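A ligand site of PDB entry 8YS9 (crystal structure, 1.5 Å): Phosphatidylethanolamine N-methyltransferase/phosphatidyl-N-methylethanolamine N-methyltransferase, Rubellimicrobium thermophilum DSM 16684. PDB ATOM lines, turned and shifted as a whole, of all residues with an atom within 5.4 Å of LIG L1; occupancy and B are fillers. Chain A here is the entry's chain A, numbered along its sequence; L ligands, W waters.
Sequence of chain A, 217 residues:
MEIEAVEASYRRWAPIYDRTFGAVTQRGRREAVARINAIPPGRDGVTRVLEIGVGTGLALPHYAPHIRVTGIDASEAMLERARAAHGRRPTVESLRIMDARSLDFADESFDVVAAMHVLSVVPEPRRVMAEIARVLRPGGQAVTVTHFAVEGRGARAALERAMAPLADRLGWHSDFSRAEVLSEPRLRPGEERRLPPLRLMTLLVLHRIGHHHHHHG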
ATOM      1  N   ILE A   3      32.928   0.837  -5.995  1.00  0.00           N
ATOM      2  CA  ILE A   3      31.713   0.052  -5.834  1.00  0.00           C
ATOM      3  C   ILE A   3      30.499   0.985  -5.627  1.00  0.00           C
ATOM      4  O   ILE A   3      29.424   0.705  -6.102  1.00  0.00           O
ATOM      5  CB  ILE A   3      31.965  -1.011  -4.736  1.00  0.00           C
ATOM      6  CG1 ILE A   3      30.964  -2.111  -4.775  1.00  0.00           C
ATOM      7  CG2 ILE A   3      32.103  -0.383  -3.354  1.00  0.00           C
ATOM      8  CD1 ILE A   3      31.176  -3.042  -5.958  1.00  0.00           C
ATOM      9  N   VAL A   6      29.414   2.127  -8.931  1.00  0.00           N
ATOM     10  CA  VAL A   6      28.699   1.044  -9.606  1.00  0.00           C
ATOM     11  C   VAL A   6      27.240   1.031  -9.153  1.00  0.00           C
ATOM     12  O   VAL A   6      26.319   1.043  -9.971  1.00  0.00           O
ATOM     13  CB  VAL A   6      29.343  -0.337  -9.388  1.00  0.00           C
ATOM     14  CG1 VAL A   6      28.463  -1.465  -9.951  1.00  0.00           C
ATOM     15  CG2 VAL A   6      30.741  -0.398  -9.937  1.00  0.00           C
ATOM     16  N   TYR A  10      24.076   1.836 -11.725  1.00  0.00           N
ATOM     17  CA  TYR A  10      23.176   0.748 -12.119  1.00  0.00           C
ATOM     18  C   TYR A  10      21.802   0.903 -11.486  1.00  0.00           C
ATOM     19  O   TYR A  10      20.848   0.332 -12.013  1.00  0.00           O
ATOM     20  CB  TYR A  10      23.837  -0.638 -11.972  1.00  0.00           C
ATOM     21  CG  TYR A  10      24.846  -0.750 -13.115  1.00  0.00           C
ATOM     22  CD1 TYR A  10      24.419  -1.152 -14.382  1.00  0.00           C
ATOM     23  CD2 TYR A  10      26.167  -0.320 -12.988  1.00  0.00           C
ATOM     24  CE1 TYR A  10      25.277  -1.130 -15.452  1.00  0.00           C
ATOM     25  CE2 TYR A  10      27.041  -0.316 -14.066  1.00  0.00           C
ATOM     26  CZ  TYR A  10      26.586  -0.715 -15.315  1.00  0.00           C
ATOM     27  OH  TYR A  10      27.407  -0.621 -16.426  1.00  0.00           O
ATOM     28  N   TYR A  17      17.626  -0.735 -18.839  1.00  0.00           N
ATOM     29  CA  TYR A  17      18.739  -1.523 -19.281  1.00  0.00           C
ATOM     30  C   TYR A  17      18.336  -2.534 -20.384  1.00  0.00           C
ATOM     31  O   TYR A  17      18.962  -2.622 -21.444  1.00  0.00           O
ATOM     32  CB  TYR A  17      19.338  -2.277 -18.074  1.00  0.00           C
ATOM     33  CG  TYR A  17      20.580  -3.072 -18.476  1.00  0.00           C
ATOM     34  CD1 TYR A  17      21.825  -2.479 -18.543  1.00  0.00           C
ATOM     35  CD2 TYR A  17      20.480  -4.419 -18.807  1.00  0.00           C
ATOM     36  CE1 TYR A  17      22.957  -3.219 -18.854  1.00  0.00           C
ATOM     37  CE2 TYR A  17      21.578  -5.148 -19.230  1.00  0.00           C
ATOM     38  CZ  TYR A  17      22.819  -4.552 -19.252  1.00  0.00           C
ATOM     39  OH  TYR A  17      23.882  -5.288 -19.605  1.00  0.00           O
ATOM     40  N   ARG A  29      25.467 -12.151 -26.032  1.00  0.00           N
ATOM     41  CA  ARG A  29      25.048 -12.834 -24.816  1.00  0.00           C
ATOM     42  C   ARG A  29      24.623 -14.278 -25.119  1.00  0.00           C
ATOM     43  O   ARG A  29      25.030 -15.243 -24.458  1.00  0.00           O
ATOM     44  CB  ARG A  29      23.995 -11.933 -24.170  1.00  0.00           C
ATOM     45  CG  ARG A  29      23.516 -12.406 -22.818  1.00  0.00           C
ATOM     46  CD  ARG A  29      22.643 -11.382 -22.131  1.00  0.00           C
ATOM     47  NE  ARG A  29      23.289 -10.092 -21.872  1.00  0.00           N
ATOM     48  CZ  ARG A  29      23.122  -8.968 -22.584  1.00  0.00           C
ATOM     49  NH1 ARG A  29      22.252  -8.865 -23.566  1.00  0.00           N
ATOM     50  NH2 ARG A  29      23.856  -7.899 -22.334  1.00  0.00           N
ATOM     51  N   GLU A  51      27.883 -16.578 -12.585  1.00  0.00           N
ATOM     52  CA  GLU A  51      27.621 -15.386 -13.390  1.00  0.00           C
ATOM     53  C   GLU A  51      28.043 -14.184 -12.554  1.00  0.00           C
ATOM     54  O   GLU A  51      27.341 -13.817 -11.610  1.00  0.00           O
ATOM     55  CB  GLU A  51      26.139 -15.288 -13.742  1.00  0.00           C
ATOM     56  CG  GLU A  51      25.780 -15.865 -15.095  1.00  0.00           C
ATOM     57  CD  GLU A  51      25.914 -14.890 -16.255  1.00  0.00           C
ATOM     58  OE1 GLU A  51      25.698 -15.285 -17.417  1.00  0.00           O
ATOM     59  OE2 GLU A  51      26.319 -13.755 -15.993  1.00  0.00           O
ATOM     60  N   ILE A  52      29.183 -13.600 -12.903  1.00  0.00           N
ATOM     61  CA  ILE A  52      29.695 -12.434 -12.209  1.00  0.00           C
ATOM     62  C   ILE A  52      29.057 -11.193 -12.841  1.00  0.00           C
ATOM     63  O   ILE A  52      29.217 -10.957 -14.024  1.00  0.00           O
ATOM     64  CB  ILE A  52      31.235 -12.381 -12.228  1.00  0.00           C
ATOM     65  CG1 ILE A  52      31.815 -13.532 -11.490  1.00  0.00           C
ATOM     66  CG2 ILE A  52      31.709 -11.059 -11.677  1.00  0.00           C
ATOM     67  CD1 ILE A  52      33.324 -13.622 -11.450  1.00  0.00           C
ATOM     68  N   GLY A  53      28.364 -10.361 -12.041  1.00  0.00           N
ATOM     69  CA  GLY A  53      27.660  -9.230 -12.633  1.00  0.00           C
ATOM     70  C   GLY A  53      26.477  -9.689 -13.473  1.00  0.00           C
ATOM     71  O   GLY A  53      26.299  -9.227 -14.597  1.00  0.00           O
ATOM     72  N   VAL A  54      25.651 -10.550 -12.929  1.00  0.00           N
ATOM     73  CA  VAL A  54      24.526 -11.146 -13.642  1.00  0.00           C
ATOM     74  C   VAL A  54      23.516 -10.080 -14.089  1.00  0.00           C
ATOM     75  O   VAL A  54      22.742 -10.338 -15.009  1.00  0.00           O
ATOM     76  CB  VAL A  54      23.891 -12.256 -12.761  1.00  0.00           C
ATOM     77  CG1 VAL A  54      23.134 -11.711 -11.550  1.00  0.00           C
ATOM     78  CG2 VAL A  54      22.971 -13.121 -13.603  1.00  0.00           C
ATOM     79  N   GLY A  55      23.495  -8.933 -13.414  1.00  0.00           N
ATOM     80  CA  GLY A  55      22.629  -7.815 -13.785  1.00  0.00           C
ATOM     81  C   GLY A  55      21.146  -8.190 -13.704  1.00  0.00           C
ATOM     82  O   GLY A  55      20.683  -8.728 -12.680  1.00  0.00           O
ATOM     83  N   THR A  56      20.411  -7.856 -14.771  1.00  0.00           N
ATOM     84  CA  THR A  56      18.990  -8.107 -14.851  1.00  0.00           C
ATOM     85  C   THR A  56      18.726  -9.560 -15.271  1.00  0.00           C
ATOM     86  O   THR A  56      17.574  -9.956 -15.411  1.00  0.00           O
ATOM     87  CB  THR A  56      18.307  -7.144 -15.823  1.00  0.00           C
ATOM     88  OG1 THR A  56      18.879  -7.387 -17.111  1.00  0.00           O
ATOM     89  CG2 THR A  56      18.468  -5.674 -15.456  1.00  0.00           C
ATOM     90  N   LEU A  58      19.621 -11.264 -18.151  1.00  0.00           N
ATOM     91  CA  LEU A  58      19.259 -11.517 -19.548  1.00  0.00           C
ATOM     92  C   LEU A  58      19.846 -12.838 -20.052  1.00  0.00           C
ATOM     93  O   LEU A  58      19.279 -13.456 -20.928  1.00  0.00           O
ATOM     94  CB  LEU A  58      19.687 -10.368 -20.455  1.00  0.00           C
ATOM     95  CG  LEU A  58      18.891  -9.059 -20.332  1.00  0.00           C
ATOM     96  CD1 LEU A  58      19.594  -7.951 -21.067  1.00  0.00           C
ATOM     97  CD2 LEU A  58      17.454  -9.275 -20.842  1.00  0.00           C
ATOM     98  N   ILE A  72      25.746 -13.340  -9.125  1.00  0.00           N
ATOM     99  CA  ILE A  72      26.050 -12.313  -8.144  1.00  0.00           C
ATOM    100  C   ILE A  72      26.068 -10.960  -8.837  1.00  0.00           C
ATOM    101  O   ILE A  72      26.352 -10.840 -10.036  1.00  0.00           O
ATOM    102  CB  ILE A  72      27.371 -12.582  -7.407  1.00  0.00           C
ATOM    103  CG1 ILE A  72      28.538 -12.560  -8.347  1.00  0.00           C
ATOM    104  CG2 ILE A  72      27.269 -13.921  -6.677  1.00  0.00           C
ATOM    105  CD1 ILE A  72      29.882 -12.380  -7.690  1.00  0.00           C
ATOM    106  N   ASP A  73      25.785  -9.923  -8.039  1.00  0.00           N
ATOM    107  CA  ASP A  73      25.812  -8.560  -8.554  1.00  0.00           C
ATOM    108  C   ASP A  73      26.028  -7.580  -7.399  1.00  0.00           C
ATOM    109  O   ASP A  73      25.722  -7.900  -6.274  1.00  0.00           O
ATOM    110  CB  ASP A  73      24.526  -8.269  -9.323  1.00  0.00           C
ATOM    111  CG  ASP A  73      24.672  -7.158 -10.337  1.00  0.00           C
ATOM    112  OD1 ASP A  73      24.498  -5.965  -9.949  1.00  0.00           O
ATOM    113  OD2 ASP A  73      24.971  -7.478 -11.493  1.00  0.00           O
ATOM    114  N   ALA A  74      26.451  -6.363  -7.728  1.00  0.00           N
ATOM    115  CA  ALA A  74      26.618  -5.291  -6.772  1.00  0.00           C
ATOM    116  C   ALA A  74      25.359  -4.437  -6.605  1.00  0.00           C
ATOM    117  O   ALA A  74      25.231  -3.700  -5.618  1.00  0.00           O
ATOM    118  CB  ALA A  74      27.817  -4.467  -7.158  1.00  0.00           C
ATOM    119  N   SER A  75      24.401  -4.556  -7.518  1.00  0.00           N
ATOM    120  CA  SER A  75      23.286  -3.621  -7.627  1.00  0.00           C
ATOM    121  C   SER A  75      21.997  -4.355  -7.277  1.00  0.00           C
ATOM    122  O   SER A  75      21.577  -5.221  -8.036  1.00  0.00           O
ATOM    123  CB  SER A  75      23.204  -3.067  -9.043  1.00  0.00           C
ATOM    124  OG  SER A  75      21.972  -2.383  -9.245  1.00  0.00           O
ATOM    125  N   MET A  78      19.423  -3.835 -10.205  1.00  0.00           N
ATOM    126  CA  MET A  78      19.591  -4.750 -11.340  1.00  0.00           C
ATOM    127  C   MET A  78      19.174  -6.154 -10.936  1.00  0.00           C
ATOM    128  O   MET A  78      18.379  -6.822 -11.613  1.00  0.00           O
ATOM    129  CB  MET A  78      21.041  -4.794 -11.864  1.00  0.00           C
ATOM    130  CG  MET A  78      21.569  -3.496 -12.401  1.00  0.00           C
ATOM    131  SD  MET A  78      20.992  -3.062 -14.071  1.00  0.00           S
ATOM    132  CE  MET A  78      22.030  -4.156 -15.074  1.00  0.00           C
ATOM    133  N   MET A  98      26.967  -9.591  -3.996  1.00  0.00           N
ATOM    134  CA  MET A  98      28.339  -9.936  -3.671  1.00  0.00           C
ATOM    135  C   MET A  98      29.260  -9.141  -4.574  1.00  0.00           C
ATOM    136  O   MET A  98      28.948  -8.945  -5.768  1.00  0.00           O
ATOM    137  CB  MET A  98      28.575 -11.439  -3.877  1.00  0.00           C
ATOM    138  CG  MET A  98      29.895 -11.924  -3.385  1.00  0.00           C
ATOM    139  SD  MET A  98      30.126 -13.679  -3.700  1.00  0.00           S
ATOM    140  CE  MET A  98      28.864 -14.403  -2.657  1.00  0.00           C
ATOM    141  N   ASP A  99      30.395  -8.723  -4.025  1.00  0.00           N
ATOM    142  CA  ASP A  99      31.402  -7.992  -4.777  1.00  0.00           C
ATOM    143  C   ASP A  99      32.363  -8.993  -5.382  1.00  0.00           C
ATOM    144  O   ASP A  99      32.965  -9.818  -4.659  1.00  0.00           O
ATOM    145  CB  ASP A  99      32.079  -6.972  -3.886  1.00  0.00           C
ATOM    146  CG  ASP A  99      33.181  -6.106  -4.466  1.00  0.00           C
ATOM    147  OD1 ASP A  99      33.637  -6.324  -5.600  1.00  0.00           O
ATOM    148  OD2 ASP A  99      33.672  -5.281  -3.669  1.00  0.00           O
ATOM    149  N   ALA A 100      32.518  -8.938  -6.711  1.00  0.00           N
ATOM    150  CA  ALA A 100      33.389  -9.853  -7.431  1.00  0.00           C
ATOM    151  C   ALA A 100      34.845  -9.809  -6.985  1.00  0.00           C
ATOM    152  O   ALA A 100      35.592 -10.725  -7.316  1.00  0.00           O
ATOM    153  CB  ALA A 100      33.292  -9.502  -8.911  1.00  0.00           C
ATOM    154  N   ARG A 101      35.274  -8.731  -6.294  1.00  0.00           N
ATOM    155  CA  ARG A 101      36.645  -8.636  -5.807  1.00  0.00           C
ATOM    156  C   ARG A 101      36.941  -9.677  -4.721  1.00  0.00           C
ATOM    157  O   ARG A 101      38.106  -9.954  -4.473  1.00  0.00           O
ATOM    158  CB  ARG A 101      36.976  -7.251  -5.253  1.00  0.00           C
ATOM    159  CG  ARG A 101      37.103  -6.184  -6.321  1.00  0.00           C
ATOM    160  CD  ARG A 101      37.285  -4.804  -5.738  1.00  0.00           C
ATOM    161  NE  ARG A 101      36.176  -4.359  -4.885  1.00  0.00           N
ATOM    162  CZ  ARG A 101      36.270  -3.294  -4.091  1.00  0.00           C
ATOM    163  NH1 ARG A 101      37.366  -2.557  -4.093  1.00  0.00           N
ATOM    164  NH2 ARG A 101      35.227  -2.941  -3.356  1.00  0.00           N
ATOM    165  N   MET A 116      29.964 -11.068 -18.515  1.00  0.00           N
ATOM    166  CA  MET A 116      29.484 -10.363 -19.715  1.00  0.00           C
ATOM    167  C   MET A 116      29.230  -8.889 -19.396  1.00  0.00           C
ATOM    168  O   MET A 116      28.415  -8.573 -18.537  1.00  0.00           O
ATOM    169  CB  MET A 116      28.233 -11.071 -20.267  1.00  0.00           C
ATOM    170  CG  MET A 116      28.367 -12.543 -20.360  1.00  0.00           C
ATOM    171  SD  MET A 116      26.877 -13.210 -21.106  1.00  0.00           S
ATOM    172  CE  MET A 116      26.985 -14.924 -20.567  1.00  0.00           C
ATOM    173  N   HIS A 117      30.040  -8.015 -20.012  1.00  0.00           N
ATOM    174  CA  HIS A 117      29.914  -6.567 -19.898  1.00  0.00           C
ATOM    175  C   HIS A 117      30.107  -6.144 -18.432  1.00  0.00           C
ATOM    176  O   HIS A 117      29.343  -5.288 -17.939  1.00  0.00           O
ATOM    177  CB  HIS A 117      28.576  -6.072 -20.495  1.00  0.00           C
ATOM    178  CG  HIS A 117      28.457  -6.551 -21.902  1.00  0.00           C
ATOM    179  ND1 HIS A 117      29.213  -6.053 -22.943  1.00  0.00           N
ATOM    180  CD2 HIS A 117      27.612  -7.471 -22.457  1.00  0.00           C
ATOM    181  CE1 HIS A 117      28.864  -6.731 -24.062  1.00  0.00           C
ATOM    182  NE2 HIS A 117      27.934  -7.585 -23.785  1.00  0.00           N
ATOM    183  N   VAL A 118      31.072  -6.780 -17.749  1.00  0.00           N
ATOM    184  CA  VAL A 118      31.254  -6.535 -16.315  1.00  0.00           C
ATOM    185  C   VAL A 118      32.715  -6.165 -16.019  1.00  0.00           C
ATOM    186  O   VAL A 118      32.968  -5.353 -15.109  1.00  0.00           O
ATOM    187  CB  VAL A 118      30.762  -7.690 -15.422  1.00  0.00           C
ATOM    188  CG1 VAL A 118      31.457  -8.992 -15.756  1.00  0.00           C
ATOM    189  CG2 VAL A 118      30.935  -7.392 -13.933  1.00  0.00           C
ATOM    190  N   VAL A 121      33.705  -2.636 -15.750  1.00  0.00           N
ATOM    191  CA  VAL A 121      32.922  -1.908 -14.757  1.00  0.00           C
ATOM    192  C   VAL A 121      33.544  -2.074 -13.355  1.00  0.00           C
ATOM    193  O   VAL A 121      33.488  -1.145 -12.522  1.00  0.00           O
ATOM    194  CB  VAL A 121      31.466  -2.380 -14.781  1.00  0.00           C
ATOM    195  CG1 VAL A 121      30.598  -1.571 -13.797  1.00  0.00           C
ATOM    196  CG2 VAL A 121      30.886  -2.376 -16.189  1.00  0.00           C
ATOM    197  N   VAL A 122      34.023  -3.283 -13.036  1.00  0.00           N
ATOM    198  CA  VAL A 122      34.428  -3.590 -11.668  1.00  0.00           C
ATOM    199  C   VAL A 122      35.529  -2.658 -11.160  1.00  0.00           C
ATOM    200  O   VAL A 122      36.408  -2.226 -11.920  1.00  0.00           O
ATOM    201  CB  VAL A 122      34.922  -5.038 -11.551  1.00  0.00           C
ATOM    202  CG1 VAL A 122      33.788  -6.007 -11.810  1.00  0.00           C
ATOM    203  CG2 VAL A 122      36.127  -5.329 -12.440  1.00  0.00           C
ATOM    204  N   PRO A 123      35.581  -2.419  -9.830  1.00  0.00           N
ATOM    205  CA  PRO A 123      36.808  -1.923  -9.217  1.00  0.00           C
ATOM    206  C   PRO A 123      37.856  -3.023  -9.248  1.00  0.00           C
ATOM    207  O   PRO A 123      37.516  -4.191  -9.150  1.00  0.00           O
ATOM    208  CB  PRO A 123      36.389  -1.596  -7.757  1.00  0.00           C
ATOM    209  CG  PRO A 123      35.075  -2.291  -7.525  1.00  0.00           C
ATOM    210  CD  PRO A 123      34.534  -2.709  -8.848  1.00  0.00           C
ATOM    211  N   VAL A 128      39.648  -9.141  -9.291  1.00  0.00           N
ATOM    212  CA  VAL A 128      38.578  -9.930  -9.857  1.00  0.00           C
ATOM    213  C   VAL A 128      39.139 -11.114 -10.671  1.00  0.00           C
ATOM    214  O   VAL A 128      38.649 -12.253 -10.516  1.00  0.00           O
ATOM    215  CB  VAL A 128      37.630  -9.063 -10.701  1.00  0.00           C
ATOM    216  CG1 VAL A 128      36.594  -9.927 -11.388  1.00  0.00           C
ATOM    217  CG2 VAL A 128      36.958  -7.994  -9.822  1.00  0.00           C
HETATM  218  N1  LIG L   1      26.054  -9.619 -17.327  1.00  0.00           N
HETATM  219  C1  LIG L   1      24.826  -8.804 -17.506  1.00  0.00           C
HETATM  220  C2  LIG L   1      24.894  -7.425 -16.814  1.00  0.00           C
HETATM  221  C3  LIG L   1      25.931  -6.456 -17.340  1.00  0.00           C
HETATM  222  S1  LIG L   1      25.779  -4.796 -16.589  1.00  0.00           S
HETATM  223  C4  LIG L   1      24.489  -8.662 -19.001  1.00  0.00           C
HETATM  224  O1  LIG L   1      25.216  -9.212 -19.854  1.00  0.00           O
HETATM  225  O2  LIG L   1      23.484  -8.011 -19.254  1.00  0.00           O
HETATM  226  C5  LIG L   1      27.157  -4.805 -15.448  1.00  0.00           C
HETATM  227  C6  LIG L   1      26.815  -5.381 -14.099  1.00  0.00           C
HETATM  228  O3  LIG L   1      28.053  -5.589 -13.362  1.00  0.00           O
HETATM  229  C7  LIG L   1      25.934  -4.484 -13.216  1.00  0.00           C
HETATM  230  O4  LIG L   1      24.709  -5.114 -12.891  1.00  0.00           O
HETATM  231  C8  LIG L   1      26.796  -4.226 -11.982  1.00  0.00           C
HETATM  232  O5  LIG L   1      26.119  -4.037 -10.767  1.00  0.00           O
HETATM  233  C9  LIG L   1      27.736  -5.425 -12.003  1.00  0.00           C
HETATM  234  N2  LIG L   1      28.992  -5.233 -11.273  1.00  0.00           N
HETATM  235  C10 LIG L   1      29.941  -4.263 -11.430  1.00  0.00           C
HETATM  236  N3  LIG L   1      30.955  -4.376 -10.606  1.00  0.00           N
HETATM  237  C11 LIG L   1      30.654  -5.476  -9.836  1.00  0.00           C
HETATM  238  C12 LIG L   1      31.311  -6.087  -8.730  1.00  0.00           C
HETATM  239  N4  LIG L   1      32.461  -5.684  -8.212  1.00  0.00           N
HETATM  240  N5  LIG L   1      30.735  -7.193  -8.224  1.00  0.00           N
HETATM  241  C13 LIG L   1      29.552  -7.569  -8.715  1.00  0.00           C
HETATM  242  N6  LIG L   1      28.821  -7.042  -9.700  1.00  0.00           N
HETATM  243  C14 LIG L   1      29.441  -5.999 -10.218  1.00  0.00           C
HETATM  244  C1  LG2 L   2      33.426   4.557 -28.675  1.00  0.00           C
HETATM  245  C2  LG2 L   2      33.376   3.813 -27.357  1.00  0.00           C
HETATM  246  C3  LG2 L   2      32.051   3.225 -27.052  1.00  0.00           C
HETATM  247  C4  LG2 L   2      32.095   2.417 -25.793  1.00  0.00           C
HETATM  248  C5  LG2 L   2      31.665   0.303 -24.817  1.00  0.00           C
HETATM  249  C6  LG2 L   2      30.324   0.406 -24.211  1.00  0.00           C
HETATM  250  C7  LG2 L   2      30.213  -0.463 -23.032  1.00  0.00           C
HETATM  251  C8  LG2 L   2      29.888  -2.405 -19.720  1.00  0.00           C
HETATM  252  C9  LG2 L   2      28.831  -1.355 -19.452  1.00  0.00           C
HETATM  253  C10 LG2 L   2      26.515  -0.739 -19.937  1.00  0.00           C
HETATM  254  C11 LG2 L   2      27.029  -2.841 -18.926  1.00  0.00           C
HETATM  255  C12 LG2 L   2      28.763   0.913 -25.951  1.00  0.00           C
HETATM  256  C13 LG2 L   2      27.813   0.266 -26.912  1.00  0.00           C
HETATM  257  C14 LG2 L   2      27.242   1.285 -27.849  1.00  0.00           C
HETATM  258  C15 LG2 L   2      25.470   6.095 -24.300  1.00  0.00           C
HETATM  259  C16 LG2 L   2      26.929   5.987 -24.585  1.00  0.00           C
HETATM  260  C17 LG2 L   2      27.289   6.550 -25.932  1.00  0.00           C
HETATM  261  C18 LG2 L   2      28.065   5.587 -26.823  1.00  0.00           C
HETATM  262  C19 LG2 L   2      28.781   6.293 -27.964  1.00  0.00           C
HETATM  263  C20 LG2 L   2      28.388   5.746 -29.313  1.00  0.00           C
HETATM  264  C21 LG2 L   2      29.342   4.735 -29.865  1.00  0.00           C
HETATM  265  C22 LG2 L   2      28.878   4.086 -31.178  1.00  0.00           C
HETATM  266  C23 LG2 L   2      29.561   4.645 -32.395  1.00  0.00           C
HETATM  267  C24 LG2 L   2      30.709   4.353 -33.003  1.00  0.00           C
HETATM  268  C25 LG2 L   2      31.670   3.281 -32.691  1.00  0.00           C
HETATM  269  C26 LG2 L   2      33.092   3.788 -32.457  1.00  0.00           C
HETATM  270  C27 LG2 L   2      33.183   4.604 -31.185  1.00  0.00           C
HETATM  271  C28 LG2 L   2      33.171   3.741 -29.918  1.00  0.00           C
HETATM  272  O1  LG2 L   2      32.391   2.865 -24.714  1.00  0.00           O
HETATM  273  O2  LG2 L   2      31.818   1.121 -26.003  1.00  0.00           O
HETATM  274  O3  LG2 L   2      30.513  -1.817 -23.298  1.00  0.00           O
HETATM  275  P1  LG2 L   2      31.056  -2.770 -22.110  1.00  0.00           P
HETATM  276  O4  LG2 L   2      32.246  -2.077 -21.500  1.00  0.00           O
HETATM  277  O5  LG2 L   2      31.302  -4.129 -22.696  1.00  0.00           O
HETATM  278  O6  LG2 L   2      29.832  -2.843 -21.084  1.00  0.00           O
HETATM  279  N1  LG2 L   2      27.490  -1.828 -19.886  1.00  0.00           N
HETATM  280  O7  LG2 L   2      29.342  -0.031 -25.182  1.00  0.00           O
HETATM  281  O8  LG2 L   2      29.024   2.081 -25.890  1.00  0.00           O
HETATM  282  C29 LG2 L   2      26.186   2.059 -27.147  1.00  0.00           C
HETATM  283  C30 LG2 L   2      24.878   1.300 -27.161  1.00  0.00           C
HETATM  284  C31 LG2 L   2      24.052   1.577 -25.932  1.00  0.00           C
HETATM  285  C32 LG2 L   2      22.577   1.731 -26.246  1.00  0.00           C
HETATM  286  C33 LG2 L   2      22.170   3.166 -25.985  1.00  0.00           C
HETATM  287  C34 LG2 L   2      21.986   3.306 -24.543  1.00  0.00           C
HETATM  288  C35 LG2 L   2      20.953   3.894 -23.980  1.00  0.00           C
HETATM  289  C36 LG2 L   2      19.888   4.635 -24.682  1.00  0.00           C
HETATM  290  C37 LG2 L   2      20.081   6.125 -24.507  1.00  0.00           C
HETATM  291  C38 LG2 L   2      20.877   6.672 -25.642  1.00  0.00           C
HETATM  292  C39 LG2 L   2      21.116   8.159 -25.547  1.00  0.00           C
HETATM  293  C40 LG2 L   2      22.583   8.507 -25.610  1.00  0.00           C
HETATM  294  C41 LG2 L   2      23.041   8.887 -27.012  1.00  0.00           C
HETATM  295  C42 LG2 L   2      23.799  10.195 -26.976  1.00  0.00           C
HETATM  296  C43 LG2 L   2      25.286   9.987 -27.088  1.00  0.00           C
HETATM  297  O   HOH W   1      28.058 -11.662 -16.464  1.00  0.00           O
HETATM  298  O   HOH W   2      25.354 -12.266 -18.178  1.00  0.00           O
HETATM  299  O   HOH W   3      21.199  -8.655 -17.650  1.00  0.00           O
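The side-chain carboxylate (OD1) of Asp 73 is in hydrogen-bond range of the backbone NH (N) of Ser 75 (2.8 Å).
The backbone NH (N) of Gly 53 is in hydrogen-bond range of the backbone carbonyl oxygen (O) of Ile 72, at 2.9 Å.
The backbone carbonyl oxygen (O) of Asp 73 lies within hydrogen-bond range of the backbone NH (N) of Met 98 (3.1 Å).
OG of Ser 75 sits at hydrogen-bond distance from N of Met 78 (3.1 Å).
The side-chain carboxylate of Asp 73 sits at hydrogen-bond distance from the backbone NH of Gly 55 (2.8 Å).
The backbone carbonyl oxygen (O) of Ile 72 sits at hydrogen-bond distance from the backbone NH (N) of Val 54 (3.0 Å).
OD2 of Asp 73 sits at hydrogen-bond distance from N of Val 54 (3.5 Å).
NH2 of Arg 101 lies within salt-bridge range of OD2 of Asp 99, at 2.8 Å.
O of Met 116 is in hydrogen-bond range of N1 of LIG L1, 2.9 Å away.
The backbone carbonyl oxygen (O) of Gly 53 sits at hydrogen-bond distance from a nitrogen (N1) of LIG L1.
An oxygen (O5) of LG2 L2 sits at hydrogen-bond distance from a ring nitrogen (ND1) of His 117.
An oxygen (O2) of LIG L1 is in hydrogen-bond range of the side-chain hydroxyl of Tyr 17, 2.8 Å away.
O1 of LIG L1 lies within salt-bridge range of NE of Arg 29, 2.9 Å away.
The backbone NH (N) of Ala 74 sits at hydrogen-bond distance from a nitrogen (N6) of LIG L1 (3.2 Å).
A nitrogen (N4) of LIG L1 sits at hydrogen-bond distance from the side-chain carboxylate of Asp 99, at 2.9 Å.
OD1 of Asp 73 lies within hydrogen-bond range of O5 of LIG L1 (2.6 Å).
N5 of LIG L1 lies within hydrogen-bond range of N of Ala 100, at 2.9 Å.
Residues that only touch LIG L1: Met 98 (3.3 Å), His 117 (3.3 Å), Val 118 (3.4 Å), Val 122 (3.5 Å), Val 6 (3.5 Å), Ser 75 (3.5 Å), Gly 55 (3.5 Å), Met 78 (3.6 Å), Val 54 (3.6 Å), Val 121 (3.6 Å), Pro 123 (3.7 Å), Ile 3 (3.7 Å) and Tyr 10 (3.8 Å).
Hydrophobic or aromatic side chains within 4 Å of LIG L1: Ile 3, Val 6, Tyr 10, Tyr 17, Ala 74, Met 78, Ala 100, Met 116, His 117, Val 118, Val 121, Val 122 and Pro 123.
Within 4 Å of LIG L1: Ile 3, Val 6, Tyr 10, Tyr 17, Arg 29, Gly 53, Val 54, Gly 55, Asp 73, Ala 74, Ser 75, Met 78, Met 98, Asp 99, Ala 100, Met 116, His 117, Val 118, Val 121, Val 122 and Pro 123.
Water W3 lies within hydrogen-bond range of the side-chain hydroxyl (OG1) of Thr 56 (2.7 Å), an oxygen (O2) of LIG L1 (2.9 Å), the backbone NH (N) of Leu 58 (3.1 Å) and the backbone carbonyl oxygen (O) of Val 54 (3.5 Å).
Water W2 lies within hydrogen-bond range of the side-chain carboxylate (OE2) of Glu 51 (2.8 Å), a nitrogen (N1) of LIG L1 (2.9 Å) and the side-chain sulfur (SD) of Met 116 (3.4 Å).
Water W1 lies within hydrogen-bond range of the side-chain carboxylate of Glu 51, the backbone carbonyl oxygen of Ile 52, the backbone NH of Met 116 and a nitrogen (N1) of LIG L1.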
